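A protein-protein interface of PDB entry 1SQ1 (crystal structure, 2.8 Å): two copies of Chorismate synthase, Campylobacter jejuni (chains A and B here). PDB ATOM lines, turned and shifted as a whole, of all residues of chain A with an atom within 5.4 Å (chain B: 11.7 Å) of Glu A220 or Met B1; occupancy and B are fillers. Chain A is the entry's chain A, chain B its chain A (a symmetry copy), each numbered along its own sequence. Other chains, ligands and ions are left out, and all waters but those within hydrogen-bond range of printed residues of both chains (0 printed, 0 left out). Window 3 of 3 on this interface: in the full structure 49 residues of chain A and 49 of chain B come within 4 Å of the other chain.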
ATOM      1  N   LEU A 218      13.168  -6.748   8.798  1.00  0.00           N
ATOM      2  CA  LEU A 218      12.053  -6.049   8.179  1.00  0.00           C
ATOM      3  C   LEU A 218      12.315  -4.542   8.215  1.00  0.00           C
ATOM      4  O   LEU A 218      12.443  -3.948   9.283  1.00  0.00           O
ATOM      5  CB  LEU A 218      10.757  -6.369   8.908  1.00  0.00           C
ATOM      6  CG  LEU A 218      10.250  -7.779   8.636  1.00  0.00           C
ATOM      7  CD1 LEU A 218       8.962  -8.026   9.397  1.00  0.00           C
ATOM      8  CD2 LEU A 218      10.019  -7.946   7.142  1.00  0.00           C
ATOM      9  N   GLY A 219      12.399  -3.923   7.043  1.00  0.00           N
ATOM     10  CA  GLY A 219      12.660  -2.501   6.978  1.00  0.00           C
ATOM     11  C   GLY A 219      13.756  -2.178   5.988  1.00  0.00           C
ATOM     12  O   GLY A 219      14.829  -2.777   6.020  1.00  0.00           O
ATOM     13  N   GLU A 220      13.473  -1.228   5.103  1.00  0.00           N
ATOM     14  CA  GLU A 220      14.413  -0.790   4.070  1.00  0.00           C
ATOM     15  C   GLU A 220      15.280   0.357   4.569  1.00  0.00           C
ATOM     16  O   GLU A 220      14.857   1.509   4.552  1.00  0.00           O
ATOM     17  CB  GLU A 220      13.644  -0.326   2.831  1.00  0.00           C
ATOM     18  CG  GLU A 220      12.996  -1.453   2.034  1.00  0.00           C
ATOM     19  CD  GLU A 220      14.020  -2.440   1.509  1.00  0.00           C
ATOM     20  OE1 GLU A 220      13.946  -3.632   1.891  1.00  0.00           O
ATOM     21  OE2 GLU A 220      14.890  -2.020   0.706  1.00  0.00           O
ATOM     22  N   VAL A 221      16.499   0.038   4.982  1.00  0.00           N
ATOM     23  CA  VAL A 221      17.400   1.045   5.511  1.00  0.00           C
ATOM     24  C   VAL A 221      17.663   2.227   4.596  1.00  0.00           C
ATOM     25  O   VAL A 221      17.699   2.114   3.359  1.00  0.00           O
ATOM     26  CB  VAL A 221      18.761   0.466   5.897  1.00  0.00           C
ATOM     27  CG1 VAL A 221      19.693   0.475   4.699  1.00  0.00           C
ATOM     28  CG2 VAL A 221      19.353   1.274   7.022  1.00  0.00           C
ATOM     29  N   LEU A 222      17.864   3.351   5.293  1.00  0.00           N
ATOM     30  CA  LEU A 222      18.125   4.688   4.794  1.00  0.00           C
ATOM     31  C   LEU A 222      16.866   5.528   4.776  1.00  0.00           C
ATOM     32  O   LEU A 222      16.634   6.290   5.715  1.00  0.00           O
ATOM     33  CB  LEU A 222      18.797   4.652   3.434  1.00  0.00           C
ATOM     34  CG  LEU A 222      20.260   5.096   3.609  1.00  0.00           C
ATOM     35  CD1 LEU A 222      20.308   6.564   3.996  1.00  0.00           C
ATOM     36  CD2 LEU A 222      20.952   4.275   4.693  1.00  0.00           C
ATOM     37  N   TYR A 223      16.030   5.384   3.754  1.00  0.00           N
ATOM     38  CA  TYR A 223      14.817   6.196   3.703  1.00  0.00           C
ATOM     39  C   TYR A 223      13.482   5.463   3.600  1.00  0.00           C
ATOM     40  O   TYR A 223      12.538   5.946   2.969  1.00  0.00           O
ATOM     41  CB  TYR A 223      14.945   7.250   2.598  1.00  0.00           C
ATOM     42  CG  TYR A 223      16.129   8.146   2.867  1.00  0.00           C
ATOM     43  CD1 TYR A 223      16.196   8.909   4.038  1.00  0.00           C
ATOM     44  CD2 TYR A 223      17.239   8.128   2.034  1.00  0.00           C
ATOM     45  CE1 TYR A 223      17.349   9.615   4.376  1.00  0.00           C
ATOM     46  CE2 TYR A 223      18.387   8.824   2.362  1.00  0.00           C
ATOM     47  CZ  TYR A 223      18.441   9.562   3.533  1.00  0.00           C
ATOM     48  OH  TYR A 223      19.604  10.223   3.854  1.00  0.00           O
ATOM     49  N   ASP A 224      13.403   4.298   4.235  1.00  0.00           N
ATOM     50  CA  ASP A 224      12.162   3.530   4.276  1.00  0.00           C
ATOM     51  C   ASP A 224      12.279   2.534   5.423  1.00  0.00           C
ATOM     52  O   ASP A 224      11.851   1.381   5.333  1.00  0.00           O
ATOM     53  CB  ASP A 224      11.880   2.817   2.946  1.00  0.00           C
ATOM     54  CG  ASP A 224      10.384   2.528   2.746  1.00  0.00           C
ATOM     55  OD1 ASP A 224       9.558   3.215   3.393  1.00  0.00           O
ATOM     56  OD2 ASP A 224      10.033   1.639   1.935  1.00  0.00           O
ATOM     57  N   LYS A 225      12.875   3.030   6.506  1.00  0.00           N
ATOM     58  CA  LYS A 225      13.103   2.285   7.731  1.00  0.00           C
ATOM     59  C   LYS A 225      11.778   1.917   8.392  1.00  0.00           C
ATOM     60  O   LYS A 225      10.788   2.638   8.271  1.00  0.00           O
ATOM     61  CB  LYS A 225      13.946   3.142   8.676  1.00  0.00           C
ATOM     62  CG  LYS A 225      15.267   3.616   8.075  1.00  0.00           C
ATOM     63  CD  LYS A 225      16.087   4.334   9.131  1.00  0.00           C
ATOM     64  CE  LYS A 225      17.544   4.460   8.738  1.00  0.00           C
ATOM     65  NZ  LYS A 225      18.339   5.111   9.829  1.00  0.00           N
ATOM     66  N   LEU A 226      11.763   0.792   9.096  1.00  0.00           N
ATOM     67  CA  LEU A 226      10.553   0.347   9.744  1.00  0.00           C
ATOM     68  C   LEU A 226      10.000   1.374  10.733  1.00  0.00           C
ATOM     69  O   LEU A 226       8.784   1.539  10.841  1.00  0.00           O
ATOM     70  CB  LEU A 226      10.783  -0.990  10.440  1.00  0.00           C
ATOM     71  CG  LEU A 226       9.485  -1.474  11.088  1.00  0.00           C
ATOM     72  CD1 LEU A 226       8.435  -1.704  10.013  1.00  0.00           C
ATOM     73  CD2 LEU A 226       9.739  -2.724  11.886  1.00  0.00           C
ATOM     74  N   GLY A 279      16.829   1.042  12.016  1.00  0.00           N
ATOM     75  CA  GLY A 279      15.720   1.150  11.088  1.00  0.00           C
ATOM     76  C   GLY A 279      15.221  -0.185  10.607  1.00  0.00           C
ATOM     77  O   GLY A 279      14.315  -0.263   9.781  1.00  0.00           O
ATOM     78  N   ILE A 280      15.821  -1.251  11.115  1.00  0.00           N
ATOM     79  CA  ILE A 280      15.401  -2.587  10.726  1.00  0.00           C
ATOM     80  C   ILE A 280      15.057  -3.316  12.019  1.00  0.00           C
ATOM     81  O   ILE A 280      15.672  -3.045  13.064  1.00  0.00           O
ATOM     82  CB  ILE A 280      16.522  -3.315   9.912  1.00  0.00           C
ATOM     83  CG1 ILE A 280      17.687  -3.708  10.808  1.00  0.00           C
ATOM     84  CG2 ILE A 280      17.059  -2.384   8.829  1.00  0.00           C
ATOM     85  CD1 ILE A 280      17.570  -5.113  11.379  1.00  0.00           C
ATOM     86  N   LEU A 346       8.839  -6.291   0.640  1.00  0.00           N
ATOM     87  CA  LEU A 346      10.007  -5.548   0.199  1.00  0.00           C
ATOM     88  C   LEU A 346      11.317  -6.262   0.481  1.00  0.00           C
ATOM     89  O   LEU A 346      12.237  -6.231  -0.327  1.00  0.00           O
ATOM     90  CB  LEU A 346      10.059  -4.194   0.887  1.00  0.00           C
ATOM     91  CG  LEU A 346       9.062  -3.148   0.417  1.00  0.00           C
ATOM     92  CD1 LEU A 346       9.221  -1.914   1.290  1.00  0.00           C
ATOM     93  CD2 LEU A 346       9.295  -2.828  -1.055  1.00  0.00           C
ATOM     94  N   ASN A 347      11.398  -6.898   1.643  1.00  0.00           N
ATOM     95  CA  ASN A 347      12.614  -7.575   2.049  1.00  0.00           C
ATOM     96  C   ASN A 347      12.740  -8.982   1.466  1.00  0.00           C
ATOM     97  O   ASN A 347      13.649  -9.736   1.817  1.00  0.00           O
ATOM     98  CB  ASN A 347      12.655  -7.636   3.568  1.00  0.00           C
ATOM     99  CG  ASN A 347      14.029  -7.915   4.094  1.00  0.00           C
ATOM    100  OD1 ASN A 347      14.919  -7.069   3.998  1.00  0.00           O
ATOM    101  ND2 ASN A 347      14.222  -9.105   4.652  1.00  0.00           N
ATOM    102  N   MET B   1      16.777   1.835  -0.096  1.00  0.00           N
ATOM    103  CA  MET B   1      16.447   3.053  -0.889  1.00  0.00           C
ATOM    104  C   MET B   1      17.255   4.183  -0.343  1.00  0.00           C
ATOM    105  O   MET B   1      17.291   4.400   0.862  1.00  0.00           O
ATOM    106  CB  MET B   1      14.977   3.441  -0.763  1.00  0.00           C
ATOM    107  CG  MET B   1      14.024   2.474  -1.394  1.00  0.00           C
ATOM    108  SD  MET B   1      14.096   0.766  -0.494  1.00  0.00           S
ATOM    109  CE  MET B   1      15.135  -0.227  -1.838  1.00  0.00           C
ATOM    110  N   ASN B   2      17.906   4.913  -1.224  1.00  0.00           N
ATOM    111  CA  ASN B   2      18.691   6.032  -0.775  1.00  0.00           C
ATOM    112  C   ASN B   2      18.103   7.309  -1.314  1.00  0.00           C
ATOM    113  O   ASN B   2      18.764   8.341  -1.327  1.00  0.00           O
ATOM    114  CB  ASN B   2      20.130   5.883  -1.228  1.00  0.00           C
ATOM    115  CG  ASN B   2      20.913   4.954  -0.344  1.00  0.00           C
ATOM    116  OD1 ASN B   2      22.139   4.951  -0.374  1.00  0.00           O
ATOM    117  ND2 ASN B   2      20.212   4.154   0.452  1.00  0.00           N
ATOM    118  N   THR B   3      16.858   7.233  -1.765  1.00  0.00           N
ATOM    119  CA  THR B   3      16.182   8.400  -2.304  1.00  0.00           C
ATOM    120  C   THR B   3      15.028   8.776  -1.390  1.00  0.00           C
ATOM    121  O   THR B   3      14.395   7.909  -0.792  1.00  0.00           O
ATOM    122  CB  THR B   3      15.649   8.139  -3.714  1.00  0.00           C
ATOM    123  OG1 THR B   3      16.741   7.815  -4.585  1.00  0.00           O
ATOM    124  CG2 THR B   3      14.939   9.373  -4.235  1.00  0.00           C
ATOM    125  N   PHE B   4      14.751  10.071  -1.296  1.00  0.00           N
ATOM    126  CA  PHE B   4      13.699  10.549  -0.422  1.00  0.00           C
ATOM    127  C   PHE B   4      12.874  11.696  -1.009  1.00  0.00           C
ATOM    128  O   PHE B   4      13.408  12.592  -1.662  1.00  0.00           O
ATOM    129  CB  PHE B   4      14.342  10.969   0.900  1.00  0.00           C
ATOM    130  CG  PHE B   4      13.393  11.593   1.881  1.00  0.00           C
ATOM    131  CD1 PHE B   4      13.511  12.934   2.211  1.00  0.00           C
ATOM    132  CD2 PHE B   4      12.415  10.830   2.508  1.00  0.00           C
ATOM    133  CE1 PHE B   4      12.669  13.512   3.152  1.00  0.00           C
ATOM    134  CE2 PHE B   4      11.566  11.398   3.456  1.00  0.00           C
ATOM    135  CZ  PHE B   4      11.694  12.742   3.781  1.00  0.00           C
ATOM    136  N   GLY B   5      11.565  11.653  -0.763  1.00  0.00           N
ATOM    137  CA  GLY B   5      10.667  12.687  -1.244  1.00  0.00           C
ATOM    138  C   GLY B   5       9.798  12.300  -2.428  1.00  0.00           C
ATOM    139  O   GLY B   5      10.164  11.431  -3.224  1.00  0.00           O
ATOM    140  N   THR B   6       8.640  12.949  -2.546  1.00  0.00           N
ATOM    141  CA  THR B   6       7.721  12.699  -3.655  1.00  0.00           C
ATOM    142  C   THR B   6       8.187  13.431  -4.914  1.00  0.00           C
ATOM    143  O   THR B   6       8.555  12.807  -5.898  1.00  0.00           O
ATOM    144  CB  THR B   6       6.314  13.203  -3.352  1.00  0.00           C
ATOM    145  OG1 THR B   6       5.899  12.742  -2.063  1.00  0.00           O
ATOM    146  CG2 THR B   6       5.354  12.695  -4.388  1.00  0.00           C
ATOM    147  N   LYS B   9      13.054  14.739  -4.711  1.00  0.00           N
ATOM    148  CA  LYS B   9      13.785  13.540  -4.342  1.00  0.00           C
ATOM    149  C   LYS B   9      15.226  13.750  -3.922  1.00  0.00           C
ATOM    150  O   LYS B   9      16.036  14.198  -4.711  1.00  0.00           O
ATOM    151  CB  LYS B   9      13.745  12.568  -5.515  1.00  0.00           C
ATOM    152  CG  LYS B   9      12.344  12.213  -5.940  1.00  0.00           C
ATOM    153  CD  LYS B   9      12.310  11.008  -6.854  1.00  0.00           C
ATOM    154  CE  LYS B   9      10.875  10.630  -7.120  1.00  0.00           C
ATOM    155  NZ  LYS B   9      10.181  10.422  -5.831  1.00  0.00           N
ATOM    156  N   PHE B  10      15.546  13.398  -2.682  1.00  0.00           N
ATOM    157  CA  PHE B  10      16.906  13.523  -2.171  1.00  0.00           C
ATOM    158  C   PHE B  10      17.566  12.156  -2.191  1.00  0.00           C
ATOM    159  O   PHE B  10      16.978  11.185  -1.731  1.00  0.00           O
ATOM    160  CB  PHE B  10      16.877  14.058  -0.742  1.00  0.00           C
ATOM    161  CG  PHE B  10      18.166  13.871   0.008  1.00  0.00           C
ATOM    162  CD1 PHE B  10      18.278  12.880   0.992  1.00  0.00           C
ATOM    163  CD2 PHE B  10      19.262  14.686  -0.245  1.00  0.00           C
ATOM    164  CE1 PHE B  10      19.462  12.708   1.718  1.00  0.00           C
ATOM    165  CE2 PHE B  10      20.451  14.522   0.474  1.00  0.00           C
ATOM    166  CZ  PHE B  10      20.548  13.531   1.458  1.00  0.00           C
ATOM    167  N   THR B  11      18.782  12.076  -2.717  1.00  0.00           N
ATOM    168  CA  THR B  11      19.484  10.802  -2.775  1.00  0.00           C
ATOM    169  C   THR B  11      20.930  10.903  -2.311  1.00  0.00           C
ATOM    170  O   THR B  11      21.694  11.741  -2.799  1.00  0.00           O
ATOM    171  CB  THR B  11      19.489  10.226  -4.205  1.00  0.00           C
ATOM    172  OG1 THR B  11      18.142  10.104  -4.668  1.00  0.00           O
ATOM    173  CG2 THR B  11      20.151   8.850  -4.235  1.00  0.00           C
ATOM    174  N   SER B  12      21.314  10.043  -1.370  1.00  0.00           N
ATOM    175  CA  SER B  12      22.688  10.047  -0.882  1.00  0.00           C
ATOM    176  C   SER B  12      23.375   8.735  -1.205  1.00  0.00           C
ATOM    177  O   SER B  12      22.829   7.659  -0.999  1.00  0.00           O
ATOM    178  CB  SER B  12      22.742  10.316   0.628  1.00  0.00           C
ATOM    179  OG  SER B  12      21.936   9.416   1.372  1.00  0.00           O
ATOM    180  N   PHE B  13      24.577   8.834  -1.749  1.00  0.00           N
ATOM    181  CA  PHE B  13      25.325   7.650  -2.091  1.00  0.00           C
ATOM    182  C   PHE B  13      26.590   7.643  -1.263  1.00  0.00           C
ATOM    183  O   PHE B  13      27.165   8.691  -0.951  1.00  0.00           O
ATOM    184  CB  PHE B  13      25.635   7.618  -3.588  1.00  0.00           C
ATOM    185  CG  PHE B  13      26.307   8.850  -4.094  1.00  0.00           C
ATOM    186  CD1 PHE B  13      27.684   8.872  -4.290  1.00  0.00           C
ATOM    187  CD2 PHE B  13      25.565   9.994  -4.371  1.00  0.00           C
ATOM    188  CE1 PHE B  13      28.318  10.018  -4.751  1.00  0.00           C
ATOM    189  CE2 PHE B  13      26.186  11.145  -4.830  1.00  0.00           C
ATOM    190  CZ  PHE B  13      27.567  11.160  -5.023  1.00  0.00           C
ATOM    191  N   GLY B  14      27.001   6.447  -0.874  1.00  0.00           N
ATOM    192  CA  GLY B  14      28.182   6.322  -0.054  1.00  0.00           C
ATOM    193  C   GLY B  14      29.439   6.063  -0.849  1.00  0.00           C
ATOM    194  O   GLY B  14      29.421   5.963  -2.077  1.00  0.00           O
ATOM    195  N   GLY B  22      28.160  11.801  -0.635  1.00  0.00           N
ATOM    196  CA  GLY B  22      27.589  12.615  -1.693  1.00  0.00           C
ATOM    197  C   GLY B  22      26.082  12.522  -1.758  1.00  0.00           C
ATOM    198  O   GLY B  22      25.501  11.508  -1.363  1.00  0.00           O
ATOM    199  N   ILE B  24      22.301  13.892  -4.060  1.00  0.00           N
ATOM    200  CA  ILE B  24      21.737  14.369  -5.316  1.00  0.00           C
ATOM    201  C   ILE B  24      20.363  14.935  -4.991  1.00  0.00           C
ATOM    202  O   ILE B  24      19.548  14.265  -4.363  1.00  0.00           O
ATOM    203  CB  ILE B  24      21.571  13.206  -6.345  1.00  0.00           C
ATOM    204  CG1 ILE B  24      22.903  12.497  -6.570  1.00  0.00           C
ATOM    205  CG2 ILE B  24      21.094  13.742  -7.683  1.00  0.00           C
ATOM    206  CD1 ILE B  24      23.982  13.394  -7.141  1.00  0.00           C
ATOM    207  N   SER B 124      28.694   1.931   4.135  1.00  0.00           N
ATOM    208  CA  SER B 124      27.492   2.505   4.741  1.00  0.00           C
ATOM    209  C   SER B 124      27.529   4.030   4.751  1.00  0.00           C
ATOM    210  O   SER B 124      26.487   4.684   4.741  1.00  0.00           O
ATOM    211  CB  SER B 124      27.335   2.018   6.186  1.00  0.00           C
ATOM    212  OG  SER B 124      27.143   0.620   6.243  1.00  0.00           O
ATOM    213  N   GLU B 127      25.839   9.218   6.279  1.00  0.00           N
ATOM    214  CA  GLU B 127      24.709   9.936   5.677  1.00  0.00           C
ATOM    215  C   GLU B 127      24.464  11.327   6.236  1.00  0.00           C
ATOM    216  O   GLU B 127      24.083  12.241   5.506  1.00  0.00           O
ATOM    217  CB  GLU B 127      23.422   9.106   5.823  1.00  0.00           C
ATOM    218  CG  GLU B 127      23.348   8.276   7.115  1.00  0.00           C
ATOM    219  CD  GLU B 127      22.093   8.531   7.952  1.00  0.00           C
ATOM    220  OE1 GLU B 127      21.941   9.646   8.498  1.00  0.00           O
ATOM    221  OE2 GLU B 127      21.258   7.609   8.074  1.00  0.00           O
ATOM    222  N   ALA B 130      25.531  14.142   4.191  1.00  0.00           N
ATOM    223  CA  ALA B 130      24.712  14.276   3.001  1.00  0.00           C
ATOM    224  C   ALA B 130      23.360  14.910   3.348  1.00  0.00           C
ATOM    225  O   ALA B 130      22.980  15.917   2.757  1.00  0.00           O
ATOM    226  CB  ALA B 130      24.516  12.908   2.353  1.00  0.00           C
ATOM    227  N   ARG B 131      22.647  14.338   4.315  1.00  0.00           N
ATOM    228  CA  ARG B 131      21.342  14.856   4.707  1.00  0.00           C
ATOM    229  C   ARG B 131      21.411  16.359   4.921  1.00  0.00           C
ATOM    230  O   ARG B 131      20.491  17.087   4.557  1.00  0.00           O
ATOM    231  CB  ARG B 131      20.868  14.168   5.985  1.00  0.00           C
ATOM    232  CG  ARG B 131      21.203  12.676   6.035  1.00  0.00           C
ATOM    233  CD  ARG B 131      20.792  12.021   7.350  1.00  0.00           C
ATOM    234  NE  ARG B 131      19.351  11.838   7.469  1.00  0.00           N
ATOM    235  CZ  ARG B 131      18.745  10.658   7.501  1.00  0.00           C
ATOM    236  NH1 ARG B 131      17.423  10.593   7.612  1.00  0.00           N
ATOM    237  NH2 ARG B 131      19.456   9.542   7.431  1.00  0.00           N
ATOM    238  N   HIS B 232       8.220  10.737   9.569  1.00  0.00           N
ATOM    239  CA  HIS B 232       8.996   9.771   8.809  1.00  0.00           C
ATOM    240  C   HIS B 232      10.443  10.240   8.665  1.00  0.00           C
ATOM    241  O   HIS B 232      11.381   9.471   8.902  1.00  0.00           O
ATOM    242  CB  HIS B 232       8.326   9.593   7.447  1.00  0.00           C
ATOM    243  CG  HIS B 232       8.972   8.589   6.547  1.00  0.00           C
ATOM    244  ND1 HIS B 232      10.290   8.692   6.146  1.00  0.00           N
ATOM    245  CD2 HIS B 232       8.454   7.547   5.857  1.00  0.00           C
ATOM    246  CE1 HIS B 232      10.546   7.762   5.237  1.00  0.00           C
ATOM    247  NE2 HIS B 232       9.447   7.059   5.046  1.00  0.00           N
ATOM    248  N   ALA B 233      10.633  11.504   8.306  1.00  0.00           N
ATOM    249  CA  ALA B 233      11.984  12.031   8.150  1.00  0.00           C
ATOM    250  C   ALA B 233      12.728  12.175   9.490  1.00  0.00           C
ATOM    251  O   ALA B 233      13.929  11.960   9.540  1.00  0.00           O
ATOM    252  CB  ALA B 233      11.944  13.364   7.414  1.00  0.00           C
ATOM    253  N   MET B 235      11.913  10.450  12.658  1.00  0.00           N
ATOM    254  CA  MET B 235      12.113   9.120  13.275  1.00  0.00           C
ATOM    255  C   MET B 235      13.234   8.412  12.528  1.00  0.00           C
ATOM    256  O   MET B 235      13.991   7.640  13.112  1.00  0.00           O
ATOM    257  CB  MET B 235      10.850   8.249  13.166  1.00  0.00           C
ATOM    258  CG  MET B 235       9.817   8.365  14.291  1.00  0.00           C
ATOM    259  SD  MET B 235      10.389   7.660  15.997  1.00  0.00           S
ATOM    260  CE  MET B 235      11.700   6.417  15.329  1.00  0.00           C
ATOM    261  N   GLY B 236      13.319   8.664  11.225  1.00  0.00           N
ATOM    262  CA  GLY B 236      14.351   8.043  10.414  1.00  0.00           C
ATOM    263  C   GLY B 236      15.768   8.418  10.825  1.00  0.00           C
ATOM    264  O   GLY B 236      16.725   7.691  10.546  1.00  0.00           O
ATOM    265  N   ILE B 237      15.903   9.564  11.483  1.00  0.00           N
ATOM    266  CA  ILE B 237      17.201  10.030  11.928  1.00  0.00           C
ATOM    267  C   ILE B 237      17.793   9.058  12.941  1.00  0.00           C
ATOM    268  O   ILE B 237      17.071   8.479  13.753  1.00  0.00           O
ATOM    269  CB  ILE B 237      17.105  11.418  12.583  1.00  0.00           C
ATOM    270  CG1 ILE B 237      16.577  12.427  11.565  1.00  0.00           C
ATOM    271  CG2 ILE B 237      18.478  11.818  13.139  1.00  0.00           C
ATOM    272  CD1 ILE B 237      16.584  13.872  12.020  1.00  0.00           C
ATOM    273  N   ASN B 238      19.108   8.880  12.890  1.00  0.00           N
ATOM    274  CA  ASN B 238      19.781   7.992  13.818  1.00  0.00           C
ATOM    275  C   ASN B 238      19.548   8.409  15.244  1.00  0.00           C
ATOM    276  O   ASN B 238      19.549   9.592  15.558  1.00  0.00           O
ATOM    277  CB  ASN B 238      21.279   7.988  13.572  1.00  0.00           C
ATOM    278  CG  ASN B 238      21.705   6.868  12.670  1.00  0.00           C
ATOM    279  OD1 ASN B 238      22.467   5.988  13.078  1.00  0.00           O
ATOM    280  ND2 ASN B 238      21.205   6.875  11.430  1.00  0.00           N
ATOM    281  N   MET B 335      16.335  17.685   7.475  1.00  0.00           N
ATOM    282  CA  MET B 335      15.207  16.830   7.136  1.00  0.00           C
ATOM    283  C   MET B 335      13.885  17.586   7.066  1.00  0.00           C
ATOM    284  O   MET B 335      13.100  17.383   6.133  1.00  0.00           O
ATOM    285  CB  MET B 335      15.069  15.671   8.136  1.00  0.00           C
ATOM    286  CG  MET B 335      16.202  14.664   8.120  1.00  0.00           C
ATOM    287  SD  MET B 335      16.690  14.035   6.351  1.00  0.00           S
ATOM    288  CE  MET B 335      15.079  13.067   5.853  1.00  0.00           C
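NZ of Lys A225 is in hydrogen-bond range of O of Gly B236, 3.1 Å away.
The side-chain hydroxyl (OG) of Ser B12 is in hydrogen-bond range of the side-chain hydroxyl (OH) of Tyr A223 (3.5 Å).
The backbone NH of Tyr A223 sits at hydrogen-bond distance from the backbone carbonyl oxygen of Met B1 (3.3 Å).
The side-chain sulfur of Met B1 sits close to the side-chain carboxylate of Glu A220, 3.1 Å away.
The backbone carbonyl oxygen (O) of Val A221 lies close to the backbone carbonyl oxygen (O) of Met B1, at 3.4 Å.
The guanidinium group of Arg B131 sits at hydrogen-bond distance from the side-chain sulfur of Met B335.
The backbone carbonyl oxygen of Glu A220 is in hydrogen-bond range of the backbone NH of Lys A225 (3.2 Å).
The backbone carbonyl oxygen (O) of Phe B4 lies within hydrogen-bond range of the backbone NH (N) of Phe B10 (2.5 Å).
The side-chain carboxylate (OE1) of Glu B127 lies within salt-bridge range of the guanidinium group (NH2) of Arg B131 (2.7 Å).
The side-chain hydroxyl (OG1) of Thr B3 is in hydrogen-bond range of the side-chain hydroxyl (OG1) of Thr B11.
OE2 of Glu B127 lies within hydrogen-bond range of ND2 of Asn B238 (3.4 Å).
Met B1 touches Leu A222 (O to CB, 3.0 Å).
Leu A222 touches Asn B2 (CG to ND2, 3.3 Å).
Asn B2 touches Tyr A223 (C to CD2, 3.6 Å).
O of Thr B3 touches CB of Tyr A223, at 3.5 Å.
CG of Tyr A223 touches CB of Phe B4, 3.9 Å away.
CE1 of Phe B10 touches OH of Tyr A223 (3.3 Å).
CE1 of Tyr A223 touches NH1 of Arg B131, at 3.4 Å.
His B232 touches Tyr A223.
ND2 of Asn B238 touches NZ of Lys A225 (3.7 Å).
Glu A220 touches just one residue of chain B: Met B1.
Of chain A, only Glu A220, Val A221, Leu A222 and Tyr A223 come within 4 Å of Met B1.
No residue of chain B comes within 4 Å of Gly A219.
Of chain B, only Met B1 and Asn B2 come within 4 Å of Leu A222.
Of the printed residues of chain B, Tyr A223 touches Met B1 (3.3 Å), Asn B2 (3.6 Å), Thr B3 (3.5 Å), Phe B4 (3.9 Å), Phe B10 (3.3 Å), Ser B12 (3.5 Å), Arg B131 (3.4 Å) and His B232 (3.5 Å).
No residue of chain B comes within 4 Å of Asp A224.
Of chain B, only Gly B236 (3.1 Å) and Asn B238 (3.7 Å) come within 4 Å of Lys A225.
No residue of chain B comes within 4 Å of Gly A279.
No residue of chain B comes within 4 Å of Asn A347.
Of the printed residues of chain A, His B232 touches Tyr A223 (3.5 Å).
Of the printed residues of chain A, Phe B10 touches Tyr A223 (3.3 Å).
Printed residues of chain A within 4 Å of Phe B4: Tyr A223 (3.9 Å).
Of the printed residues of chain A, Arg B131 touches Tyr A223.
Of the printed residues of chain A, Gly B236 touches Lys A225.
Met B335 touches none of the printed residues of chain A.
The nearest residue of chain B that does not touch Glu A220 is Asn B2 (7.2 Å).
Along chain B the printed residues that touch a printed residue of chain A span positions 1 to 238.
Hydrophobic or aromatic side chains of chain A within 4 Å of the printed part of chain B: Leu A222 and Tyr A223.
Among the printed residues, no Asp or Glu carboxylate lies within 4 Å of a Lys or Arg side-chain nitrogen of the other chain.
No position is printed for both chains.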
